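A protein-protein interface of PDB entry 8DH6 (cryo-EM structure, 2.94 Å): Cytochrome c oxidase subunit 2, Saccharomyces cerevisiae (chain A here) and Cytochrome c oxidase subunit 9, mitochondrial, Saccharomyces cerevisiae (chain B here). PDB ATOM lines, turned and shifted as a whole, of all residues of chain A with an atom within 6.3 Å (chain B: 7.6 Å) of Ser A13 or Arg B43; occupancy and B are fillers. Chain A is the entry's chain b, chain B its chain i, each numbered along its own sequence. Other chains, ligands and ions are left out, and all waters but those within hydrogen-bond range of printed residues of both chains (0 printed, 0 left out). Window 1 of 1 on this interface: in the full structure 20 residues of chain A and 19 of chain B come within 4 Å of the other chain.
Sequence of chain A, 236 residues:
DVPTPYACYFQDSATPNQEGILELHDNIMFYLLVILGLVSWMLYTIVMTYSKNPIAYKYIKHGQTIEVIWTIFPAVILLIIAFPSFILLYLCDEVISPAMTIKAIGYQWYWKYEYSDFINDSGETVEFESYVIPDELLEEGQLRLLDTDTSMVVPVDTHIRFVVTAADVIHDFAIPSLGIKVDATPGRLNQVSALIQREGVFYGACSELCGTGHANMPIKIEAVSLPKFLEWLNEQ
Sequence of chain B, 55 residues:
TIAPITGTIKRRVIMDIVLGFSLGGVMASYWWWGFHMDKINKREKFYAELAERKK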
ATOM      1  N   ASP A   1     -20.968 -24.813  23.004  1.00  0.00           N
ATOM      2  CA  ASP A   1     -20.160 -25.345  21.914  1.00  0.00           C
ATOM      3  C   ASP A   1     -20.907 -26.454  21.191  1.00  0.00           C
ATOM      4  O   ASP A   1     -21.019 -26.449  19.967  1.00  0.00           O
ATOM      5  CB  ASP A   1     -18.825 -25.866  22.441  1.00  0.00           C
ATOM      6  CG  ASP A   1     -18.037 -24.802  23.174  1.00  0.00           C
ATOM      7  OD1 ASP A   1     -18.263 -23.606  22.900  1.00  0.00           O
ATOM      8  OD2 ASP A   1     -17.193 -25.155  24.021  1.00  0.00           O
ATOM      9  N   GLN A  11     -25.947 -22.386  24.620  1.00  0.00           N
ATOM     10  CA  GLN A  11     -24.655 -23.046  24.657  1.00  0.00           C
ATOM     11  C   GLN A  11     -23.594 -22.068  25.153  1.00  0.00           C
ATOM     12  O   GLN A  11     -23.773 -20.846  25.123  1.00  0.00           O
ATOM     13  CB  GLN A  11     -24.289 -23.592  23.279  1.00  0.00           C
ATOM     14  CG  GLN A  11     -25.443 -24.253  22.554  1.00  0.00           C
ATOM     15  CD  GLN A  11     -25.009 -24.953  21.287  1.00  0.00           C
ATOM     16  OE1 GLN A  11     -23.818 -25.058  21.000  1.00  0.00           O
ATOM     17  NE2 GLN A  11     -25.975 -25.443  20.521  1.00  0.00           N
ATOM     18  N   ASP A  12     -22.481 -22.617  25.628  1.00  0.00           N
ATOM     19  CA  ASP A  12     -21.429 -21.784  26.194  1.00  0.00           C
ATOM     20  C   ASP A  12     -20.863 -20.849  25.133  1.00  0.00           C
ATOM     21  O   ASP A  12     -20.557 -21.270  24.014  1.00  0.00           O
ATOM     22  CB  ASP A  12     -20.328 -22.656  26.789  1.00  0.00           C
ATOM     23  CG  ASP A  12     -20.704 -23.212  28.144  1.00  0.00           C
ATOM     24  OD1 ASP A  12     -21.802 -22.880  28.632  1.00  0.00           O
ATOM     25  OD2 ASP A  12     -19.902 -23.968  28.729  1.00  0.00           O
ATOM     26  N   SER A  13     -20.732 -19.575  25.489  1.00  0.00           N
ATOM     27  CA  SER A  13     -20.307 -18.559  24.542  1.00  0.00           C
ATOM     28  C   SER A  13     -18.811 -18.662  24.262  1.00  0.00           C
ATOM     29  O   SER A  13     -18.029 -19.174  25.066  1.00  0.00           O
ATOM     30  CB  SER A  13     -20.636 -17.167  25.072  1.00  0.00           C
ATOM     31  OG  SER A  13     -19.693 -16.760  26.045  1.00  0.00           O
ATOM     32  N   ALA A  14     -18.417 -18.163  23.089  1.00  0.00           N
ATOM     33  CA  ALA A  14     -17.006 -18.060  22.748  1.00  0.00           C
ATOM     34  C   ALA A  14     -16.667 -16.738  22.074  1.00  0.00           C
ATOM     35  O   ALA A  14     -15.487 -16.481  21.813  1.00  0.00           O
ATOM     36  CB  ALA A  14     -16.581 -19.217  21.846  1.00  0.00           C
ATOM     37  N   THR A  15     -17.656 -15.897  21.787  1.00  0.00           N
ATOM     38  CA  THR A  15     -17.432 -14.604  21.158  1.00  0.00           C
ATOM     39  C   THR A  15     -18.165 -13.548  21.969  1.00  0.00           C
ATOM     40  O   THR A  15     -19.138 -13.861  22.663  1.00  0.00           O
ATOM     41  CB  THR A  15     -17.922 -14.593  19.700  1.00  0.00           C
ATOM     42  OG1 THR A  15     -19.353 -14.632  19.673  1.00  0.00           O
ATOM     43  CG2 THR A  15     -17.372 -15.778  18.932  1.00  0.00           C
ATOM     44  N   GLN A  18     -22.090 -13.490  21.420  1.00  0.00           N
ATOM     45  CA  GLN A  18     -22.958 -14.459  22.081  1.00  0.00           C
ATOM     46  C   GLN A  18     -23.192 -14.091  23.538  1.00  0.00           C
ATOM     47  O   GLN A  18     -24.324 -14.168  24.027  1.00  0.00           O
ATOM     48  CB  GLN A  18     -22.368 -15.862  21.969  1.00  0.00           C
ATOM     49  CG  GLN A  18     -23.213 -16.937  22.634  1.00  0.00           C
ATOM     50  CD  GLN A  18     -24.685 -16.819  22.295  1.00  0.00           C
ATOM     51  OE1 GLN A  18     -25.086 -16.998  21.147  1.00  0.00           O
ATOM     52  NE2 GLN A  18     -25.499 -16.526  23.299  1.00  0.00           N
ATOM     53  N   GLU A  19     -22.145 -13.676  24.251  1.00  0.00           N
ATOM     54  CA  GLU A  19     -22.343 -13.272  25.637  1.00  0.00           C
ATOM     55  C   GLU A  19     -23.114 -11.964  25.746  1.00  0.00           C
ATOM     56  O   GLU A  19     -23.895 -11.797  26.690  1.00  0.00           O
ATOM     57  CB  GLU A  19     -21.000 -13.179  26.360  1.00  0.00           C
ATOM     58  CG  GLU A  19     -20.006 -12.215  25.760  1.00  0.00           C
ATOM     59  CD  GLU A  19     -18.598 -12.463  26.264  1.00  0.00           C
ATOM     60  OE1 GLU A  19     -18.268 -13.635  26.536  1.00  0.00           O
ATOM     61  OE2 GLU A  19     -17.827 -11.492  26.399  1.00  0.00           O
ATOM     62  N   LEU A  22     -26.665 -12.964  25.214  1.00  0.00           N
ATOM     63  CA  LEU A  22     -27.101 -13.687  26.404  1.00  0.00           C
ATOM     64  C   LEU A  22     -27.460 -12.725  27.531  1.00  0.00           C
ATOM     65  O   LEU A  22     -28.497 -12.877  28.192  1.00  0.00           O
ATOM     66  CB  LEU A  22     -26.001 -14.653  26.840  1.00  0.00           C
ATOM     67  CG  LEU A  22     -26.218 -15.542  28.060  1.00  0.00           C
ATOM     68  CD1 LEU A  22     -25.726 -16.941  27.763  1.00  0.00           C
ATOM     69  CD2 LEU A  22     -25.486 -14.974  29.258  1.00  0.00           C
ATOM     70  N   GLU A  23     -26.610 -11.721  27.762  1.00  0.00           N
ATOM     71  CA  GLU A  23     -26.912 -10.712  28.771  1.00  0.00           C
ATOM     72  C   GLU A  23     -28.170  -9.931  28.417  1.00  0.00           C
ATOM     73  O   GLU A  23     -28.986  -9.640  29.299  1.00  0.00           O
ATOM     74  CB  GLU A  23     -25.723  -9.767  28.939  1.00  0.00           C
ATOM     75  CG  GLU A  23     -25.797  -8.879  30.167  1.00  0.00           C
ATOM     76  CD  GLU A  23     -26.521  -7.576  29.904  1.00  0.00           C
ATOM     77  OE1 GLU A  23     -26.497  -7.106  28.747  1.00  0.00           O
ATOM     78  OE2 GLU A  23     -27.112  -7.021  30.852  1.00  0.00           O
ATOM     79  N   PRO A 176     -24.537 -21.183  16.887  1.00  0.00           N
ATOM     80  CA  PRO A 176     -25.066 -20.525  18.087  1.00  0.00           C
ATOM     81  C   PRO A 176     -24.028 -20.275  19.166  1.00  0.00           C
ATOM     82  O   PRO A 176     -24.130 -19.260  19.865  1.00  0.00           O
ATOM     83  CB  PRO A 176     -26.140 -21.504  18.574  1.00  0.00           C
ATOM     84  CG  PRO A 176     -25.671 -22.828  18.094  1.00  0.00           C
ATOM     85  CD  PRO A 176     -24.987 -22.582  16.779  1.00  0.00           C
ATOM     86  N   SER A 177     -23.040 -21.156  19.324  1.00  0.00           N
ATOM     87  CA  SER A 177     -22.018 -20.946  20.342  1.00  0.00           C
ATOM     88  C   SER A 177     -21.187 -19.701  20.066  1.00  0.00           C
ATOM     89  O   SER A 177     -20.813 -18.994  21.006  1.00  0.00           O
ATOM     90  CB  SER A 177     -21.112 -22.170  20.438  1.00  0.00           C
ATOM     91  OG  SER A 177     -20.096 -21.966  21.402  1.00  0.00           O
ATOM     92  N   LEU A 178     -20.882 -19.426  18.802  1.00  0.00           N
ATOM     93  CA  LEU A 178     -20.227 -18.184  18.419  1.00  0.00           C
ATOM     94  C   LEU A 178     -21.204 -17.027  18.300  1.00  0.00           C
ATOM     95  O   LEU A 178     -20.774 -15.886  18.105  1.00  0.00           O
ATOM     96  CB  LEU A 178     -19.480 -18.355  17.094  1.00  0.00           C
ATOM     97  CG  LEU A 178     -18.429 -19.458  17.020  1.00  0.00           C
ATOM     98  CD1 LEU A 178     -17.695 -19.388  15.695  1.00  0.00           C
ATOM     99  CD2 LEU A 178     -17.465 -19.355  18.180  1.00  0.00           C
ATOM    100  N   GLN A 197     -12.808 -16.483  21.643  1.00  0.00           N
ATOM    101  CA  GLN A 197     -12.020 -16.207  22.835  1.00  0.00           C
ATOM    102  C   GLN A 197     -11.380 -17.445  23.446  1.00  0.00           C
ATOM    103  O   GLN A 197     -10.496 -17.307  24.296  1.00  0.00           O
ATOM    104  CB  GLN A 197     -12.895 -15.518  23.888  1.00  0.00           C
ATOM    105  CG  GLN A 197     -13.350 -14.131  23.478  1.00  0.00           C
ATOM    106  CD  GLN A 197     -14.229 -13.474  24.517  1.00  0.00           C
ATOM    107  OE1 GLN A 197     -14.567 -14.076  25.534  1.00  0.00           O
ATOM    108  NE2 GLN A 197     -14.605 -12.227  24.266  1.00  0.00           N
ATOM    109  N   ARG A 198     -11.793 -18.642  23.039  1.00  0.00           N
ATOM    110  CA  ARG A 198     -11.239 -19.863  23.598  1.00  0.00           C
ATOM    111  C   ARG A 198     -11.177 -20.929  22.516  1.00  0.00           C
ATOM    112  O   ARG A 198     -12.057 -21.016  21.657  1.00  0.00           O
ATOM    113  CB  ARG A 198     -12.070 -20.365  24.783  1.00  0.00           C
ATOM    114  CG  ARG A 198     -13.538 -20.551  24.466  1.00  0.00           C
ATOM    115  CD  ARG A 198     -14.309 -21.026  25.678  1.00  0.00           C
ATOM    116  NE  ARG A 198     -15.737 -21.108  25.402  1.00  0.00           N
ATOM    117  CZ  ARG A 198     -16.342 -22.183  24.918  1.00  0.00           C
ATOM    118  NH1 ARG A 198     -15.671 -23.289  24.644  1.00  0.00           N
ATOM    119  NH2 ARG A 198     -17.653 -22.146  24.702  1.00  0.00           N
ATOM    120  N   PHE A 202     -16.900 -25.947  17.754  1.00  0.00           N
ATOM    121  CA  PHE A 202     -18.179 -25.251  17.789  1.00  0.00           C
ATOM    122  C   PHE A 202     -19.047 -25.790  16.668  1.00  0.00           C
ATOM    123  O   PHE A 202     -18.654 -25.748  15.498  1.00  0.00           O
ATOM    124  CB  PHE A 202     -17.984 -23.739  17.649  1.00  0.00           C
ATOM    125  CG  PHE A 202     -16.938 -23.180  18.569  1.00  0.00           C
ATOM    126  CD1 PHE A 202     -17.204 -23.000  19.912  1.00  0.00           C
ATOM    127  CD2 PHE A 202     -15.682 -22.852  18.092  1.00  0.00           C
ATOM    128  CE1 PHE A 202     -16.243 -22.494  20.759  1.00  0.00           C
ATOM    129  CE2 PHE A 202     -14.716 -22.345  18.935  1.00  0.00           C
ATOM    130  CZ  PHE A 202     -14.997 -22.166  20.271  1.00  0.00           C
ATOM    131  N   HIS B  36     -28.662 -16.108  36.276  1.00  0.00           N
ATOM    132  CA  HIS B  36     -27.814 -15.334  35.382  1.00  0.00           C
ATOM    133  C   HIS B  36     -26.476 -15.035  36.035  1.00  0.00           C
ATOM    134  O   HIS B  36     -25.425 -15.121  35.388  1.00  0.00           O
ATOM    135  CB  HIS B  36     -28.520 -14.039  34.985  1.00  0.00           C
ATOM    136  CG  HIS B  36     -27.635 -13.061  34.281  1.00  0.00           C
ATOM    137  ND1 HIS B  36     -27.093 -13.309  33.038  1.00  0.00           N
ATOM    138  CD2 HIS B  36     -27.185 -11.840  34.649  1.00  0.00           C
ATOM    139  CE1 HIS B  36     -26.358 -12.277  32.667  1.00  0.00           C
ATOM    140  NE2 HIS B  36     -26.394 -11.372  33.628  1.00  0.00           N
ATOM    141  N   MET B  37     -26.494 -14.701  37.325  1.00  0.00           N
ATOM    142  CA  MET B  37     -25.250 -14.393  38.013  1.00  0.00           C
ATOM    143  C   MET B  37     -24.394 -15.635  38.214  1.00  0.00           C
ATOM    144  O   MET B  37     -23.167 -15.534  38.188  1.00  0.00           O
ATOM    145  CB  MET B  37     -25.535 -13.705  39.344  1.00  0.00           C
ATOM    146  CG  MET B  37     -26.173 -12.340  39.181  1.00  0.00           C
ATOM    147  SD  MET B  37     -25.126 -11.193  38.267  1.00  0.00           S
ATOM    148  CE  MET B  37     -23.805 -10.932  39.444  1.00  0.00           C
ATOM    149  N   ASP B  38     -25.001 -16.814  38.386  1.00  0.00           N
ATOM    150  CA  ASP B  38     -24.202 -18.033  38.430  1.00  0.00           C
ATOM    151  C   ASP B  38     -23.517 -18.292  37.095  1.00  0.00           C
ATOM    152  O   ASP B  38     -22.331 -18.642  37.058  1.00  0.00           O
ATOM    153  CB  ASP B  38     -25.074 -19.221  38.826  1.00  0.00           C
ATOM    154  CG  ASP B  38     -24.259 -20.413  39.284  1.00  0.00           C
ATOM    155  OD1 ASP B  38     -23.066 -20.231  39.609  1.00  0.00           O
ATOM    156  OD2 ASP B  38     -24.809 -21.533  39.320  1.00  0.00           O
ATOM    157  N   LYS B  39     -24.244 -18.120  35.987  1.00  0.00           N
ATOM    158  CA  LYS B  39     -23.615 -18.313  34.681  1.00  0.00           C
ATOM    159  C   LYS B  39     -22.485 -17.312  34.457  1.00  0.00           C
ATOM    160  O   LYS B  39     -21.405 -17.681  33.974  1.00  0.00           O
ATOM    161  CB  LYS B  39     -24.653 -18.208  33.566  1.00  0.00           C
ATOM    162  CG  LYS B  39     -25.874 -19.089  33.754  1.00  0.00           C
ATOM    163  CD  LYS B  39     -25.505 -20.553  33.924  1.00  0.00           C
ATOM    164  CE  LYS B  39     -25.124 -21.190  32.599  1.00  0.00           C
ATOM    165  NZ  LYS B  39     -24.926 -22.661  32.725  1.00  0.00           N
ATOM    166  N   ILE B  40     -22.712 -16.045  34.816  1.00  0.00           N
ATOM    167  CA  ILE B  40     -21.683 -15.023  34.637  1.00  0.00           C
ATOM    168  C   ILE B  40     -20.472 -15.318  35.513  1.00  0.00           C
ATOM    169  O   ILE B  40     -19.324 -15.155  35.084  1.00  0.00           O
ATOM    170  CB  ILE B  40     -22.258 -13.625  34.925  1.00  0.00           C
ATOM    171  CG1 ILE B  40     -23.381 -13.296  33.946  1.00  0.00           C
ATOM    172  CG2 ILE B  40     -21.168 -12.573  34.840  1.00  0.00           C
ATOM    173  CD1 ILE B  40     -22.946 -13.259  32.513  1.00  0.00           C
ATOM    174  N   ASN B  41     -20.707 -15.742  36.757  1.00  0.00           N
ATOM    175  CA  ASN B  41     -19.607 -16.068  37.655  1.00  0.00           C
ATOM    176  C   ASN B  41     -18.790 -17.236  37.124  1.00  0.00           C
ATOM    177  O   ASN B  41     -17.555 -17.203  37.166  1.00  0.00           O
ATOM    178  CB  ASN B  41     -20.151 -16.385  39.048  1.00  0.00           C
ATOM    179  CG  ASN B  41     -20.576 -15.143  39.804  1.00  0.00           C
ATOM    180  OD1 ASN B  41     -20.048 -14.055  39.580  1.00  0.00           O
ATOM    181  ND2 ASN B  41     -21.544 -15.299  40.696  1.00  0.00           N
ATOM    182  N   LYS B  42     -19.459 -18.276  36.617  1.00  0.00           N
ATOM    183  CA  LYS B  42     -18.738 -19.403  36.036  1.00  0.00           C
ATOM    184  C   LYS B  42     -17.904 -18.968  34.839  1.00  0.00           C
ATOM    185  O   LYS B  42     -16.736 -19.356  34.713  1.00  0.00           O
ATOM    186  CB  LYS B  42     -19.716 -20.502  35.630  1.00  0.00           C
ATOM    187  CG  LYS B  42     -20.421 -21.172  36.789  1.00  0.00           C
ATOM    188  CD  LYS B  42     -21.331 -22.281  36.301  1.00  0.00           C
ATOM    189  CE  LYS B  42     -22.099 -22.901  37.450  1.00  0.00           C
ATOM    190  NZ  LYS B  42     -21.200 -23.640  38.377  1.00  0.00           N
ATOM    191  N   ARG B  43     -18.485 -18.156  33.950  1.00  0.00           N
ATOM    192  CA  ARG B  43     -17.741 -17.705  32.778  1.00  0.00           C
ATOM    193  C   ARG B  43     -16.528 -16.871  33.172  1.00  0.00           C
ATOM    194  O   ARG B  43     -15.426 -17.076  32.645  1.00  0.00           O
ATOM    195  CB  ARG B  43     -18.654 -16.905  31.852  1.00  0.00           C
ATOM    196  CG  ARG B  43     -18.001 -16.558  30.534  1.00  0.00           C
ATOM    197  CD  ARG B  43     -18.941 -15.820  29.605  1.00  0.00           C
ATOM    198  NE  ARG B  43     -19.109 -14.427  29.994  1.00  0.00           N
ATOM    199  CZ  ARG B  43     -20.284 -13.832  30.138  1.00  0.00           C
ATOM    200  NH1 ARG B  43     -21.416 -14.477  29.911  1.00  0.00           N
ATOM    201  NH2 ARG B  43     -20.324 -12.557  30.513  1.00  0.00           N
ATOM    202  N   GLU B  44     -16.710 -15.928  34.099  1.00  0.00           N
ATOM    203  CA  GLU B  44     -15.601 -15.089  34.533  1.00  0.00           C
ATOM    204  C   GLU B  44     -14.518 -15.903  35.222  1.00  0.00           C
ATOM    205  O   GLU B  44     -13.328 -15.659  34.998  1.00  0.00           O
ATOM    206  CB  GLU B  44     -16.110 -13.987  35.460  1.00  0.00           C
ATOM    207  CG  GLU B  44     -16.962 -12.937  34.765  1.00  0.00           C
ATOM    208  CD  GLU B  44     -16.207 -12.203  33.675  1.00  0.00           C
ATOM    209  OE1 GLU B  44     -15.070 -11.754  33.936  1.00  0.00           O
ATOM    210  OE2 GLU B  44     -16.750 -12.074  32.557  1.00  0.00           O
ATOM    211  N   LYS B  45     -14.905 -16.872  36.055  1.00  0.00           N
ATOM    212  CA  LYS B  45     -13.923 -17.721  36.720  1.00  0.00           C
ATOM    213  C   LYS B  45     -13.127 -18.537  35.709  1.00  0.00           C
ATOM    214  O   LYS B  45     -11.896 -18.638  35.811  1.00  0.00           O
ATOM    215  CB  LYS B  45     -14.633 -18.633  37.720  1.00  0.00           C
ATOM    216  CG  LYS B  45     -13.719 -19.462  38.598  1.00  0.00           C
ATOM    217  CD  LYS B  45     -14.531 -20.321  39.556  1.00  0.00           C
ATOM    218  CE  LYS B  45     -13.635 -21.084  40.518  1.00  0.00           C
ATOM    219  NZ  LYS B  45     -12.651 -21.942  39.803  1.00  0.00           N
ATOM    220  N   PHE B  46     -13.809 -19.115  34.715  1.00  0.00           N
ATOM    221  CA  PHE B  46     -13.104 -19.889  33.699  1.00  0.00           C
ATOM    222  C   PHE B  46     -12.143 -19.016  32.903  1.00  0.00           C
ATOM    223  O   PHE B  46     -11.006 -19.419  32.633  1.00  0.00           O
ATOM    224  CB  PHE B  46     -14.095 -20.566  32.756  1.00  0.00           C
ATOM    225  CG  PHE B  46     -13.467 -21.060  31.485  1.00  0.00           C
ATOM    226  CD1 PHE B  46     -12.625 -22.157  31.494  1.00  0.00           C
ATOM    227  CD2 PHE B  46     -13.702 -20.414  30.286  1.00  0.00           C
ATOM    228  CE1 PHE B  46     -12.040 -22.608  30.329  1.00  0.00           C
ATOM    229  CE2 PHE B  46     -13.119 -20.861  29.119  1.00  0.00           C
ATOM    230  CZ  PHE B  46     -12.289 -21.958  29.140  1.00  0.00           C
ATOM    231  N   TYR B  47     -12.582 -17.818  32.512  1.00  0.00           N
ATOM    232  CA  TYR B  47     -11.710 -16.953  31.726  1.00  0.00           C
ATOM    233  C   TYR B  47     -10.531 -16.449  32.549  1.00  0.00           C
ATOM    234  O   TYR B  47      -9.425 -16.301  32.016  1.00  0.00           O
ATOM    235  CB  TYR B  47     -12.510 -15.788  31.149  1.00  0.00           C
ATOM    236  CG  TYR B  47     -13.285 -16.160  29.907  1.00  0.00           C
ATOM    237  CD1 TYR B  47     -12.803 -17.117  29.027  1.00  0.00           C
ATOM    238  CD2 TYR B  47     -14.502 -15.564  29.621  1.00  0.00           C
ATOM    239  CE1 TYR B  47     -13.509 -17.464  27.894  1.00  0.00           C
ATOM    240  CE2 TYR B  47     -15.215 -15.905  28.491  1.00  0.00           C
ATOM    241  CZ  TYR B  47     -14.714 -16.855  27.632  1.00  0.00           C
ATOM    242  OH  TYR B  47     -15.425 -17.192  26.507  1.00  0.00           O
ATOM    243  N   ALA B  48     -10.739 -16.194  33.842  1.00  0.00           N
ATOM    244  CA  ALA B  48      -9.626 -15.827  34.711  1.00  0.00           C
ATOM    245  C   ALA B  48      -8.619 -16.964  34.823  1.00  0.00           C
ATOM    246  O   ALA B  48      -7.407 -16.730  34.774  1.00  0.00           O
ATOM    247  CB  ALA B  48     -10.144 -15.430  36.091  1.00  0.00           C
ATOM    248  N   GLU B  49      -9.100 -18.201  34.970  1.00  0.00           N
ATOM    249  CA  GLU B  49      -8.186 -19.340  35.010  1.00  0.00           C
ATOM    250  C   GLU B  49      -7.431 -19.500  33.696  1.00  0.00           C
ATOM    251  O   GLU B  49      -6.238 -19.828  33.699  1.00  0.00           O
ATOM    252  CB  GLU B  49      -8.951 -20.620  35.339  1.00  0.00           C
ATOM    253  CG  GLU B  49      -9.467 -20.687  36.763  1.00  0.00           C
ATOM    254  CD  GLU B  49     -10.518 -21.763  36.949  1.00  0.00           C
ATOM    255  OE1 GLU B  49     -10.534 -22.725  36.153  1.00  0.00           O
ATOM    256  OE2 GLU B  49     -11.331 -21.647  37.891  1.00  0.00           O
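Ser A13 touches Arg B43 (OG to CD, 3.8 Å).
Ser A13 touches Tyr B47 (O to OH, 3.6 Å).
CE2 of Phe B46 touches CD of Arg A198 (3.6 Å).
OE1 of Gln A197 sits at hydrogen-bond distance from OH of Tyr B47 (3.4 Å).
OE1 of Glu A19 lies within salt-bridge range of NE of Arg B43, at 3.6 Å.
Ser A13 touches two residues of chain B.
Thr A15 touches none of the printed residues of chain B.
Printed residues of chain B within 4 Å of Gln A197: Tyr B47.
Of the printed residues of chain B, Arg A198 touches Phe B46.
Of chain A, only Ser A13 and Glu A19 come within 4 Å of Arg B43.
Of the printed residues of chain A, Tyr B47 touches Ser A13 (3.6 Å) and Gln A197 (3.4 Å).
The nearest residue of chain B that does not touch Ser A13 is Phe B46 (6.6 Å).
Of the 16 printed residues of chain A, 4 touch a printed residue of chain B.
Along chain A the printed residues that touch a printed residue of chain B span positions 13 to 198.
Of the 14 printed residues of chain B, 3 touch a printed residue of chain A.
Hydrophobic or aromatic side chains of chain B that line the printed part of chain A: Phe B46 and Tyr B47.
Among the printed residues, Asp or Glu carboxylates within 4 Å of a Lys or Arg side-chain nitrogen of the other chain: Glu A19 with Arg B43 (3.6 Å).
The side-chain carboxylate of Asp A1 is in salt-bridge range of the guanidinium group of Arg A198 (2.5 Å).
O of Ala A14 is in hydrogen-bond range of N of Gln A197 (2.7 Å).
The guanidinium group (NH2) of Arg A198 sits at hydrogen-bond distance from the backbone carbonyl oxygen (O) of Asp A12 (3.1 Å).
The guanidinium group (NH2) of Arg A198 lies within hydrogen-bond range of the backbone carbonyl oxygen (O) of Ser A13 (3.0 Å).
OG of Ser A13 sits at hydrogen-bond distance from OE1 of Glu A19 (3.5 Å).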
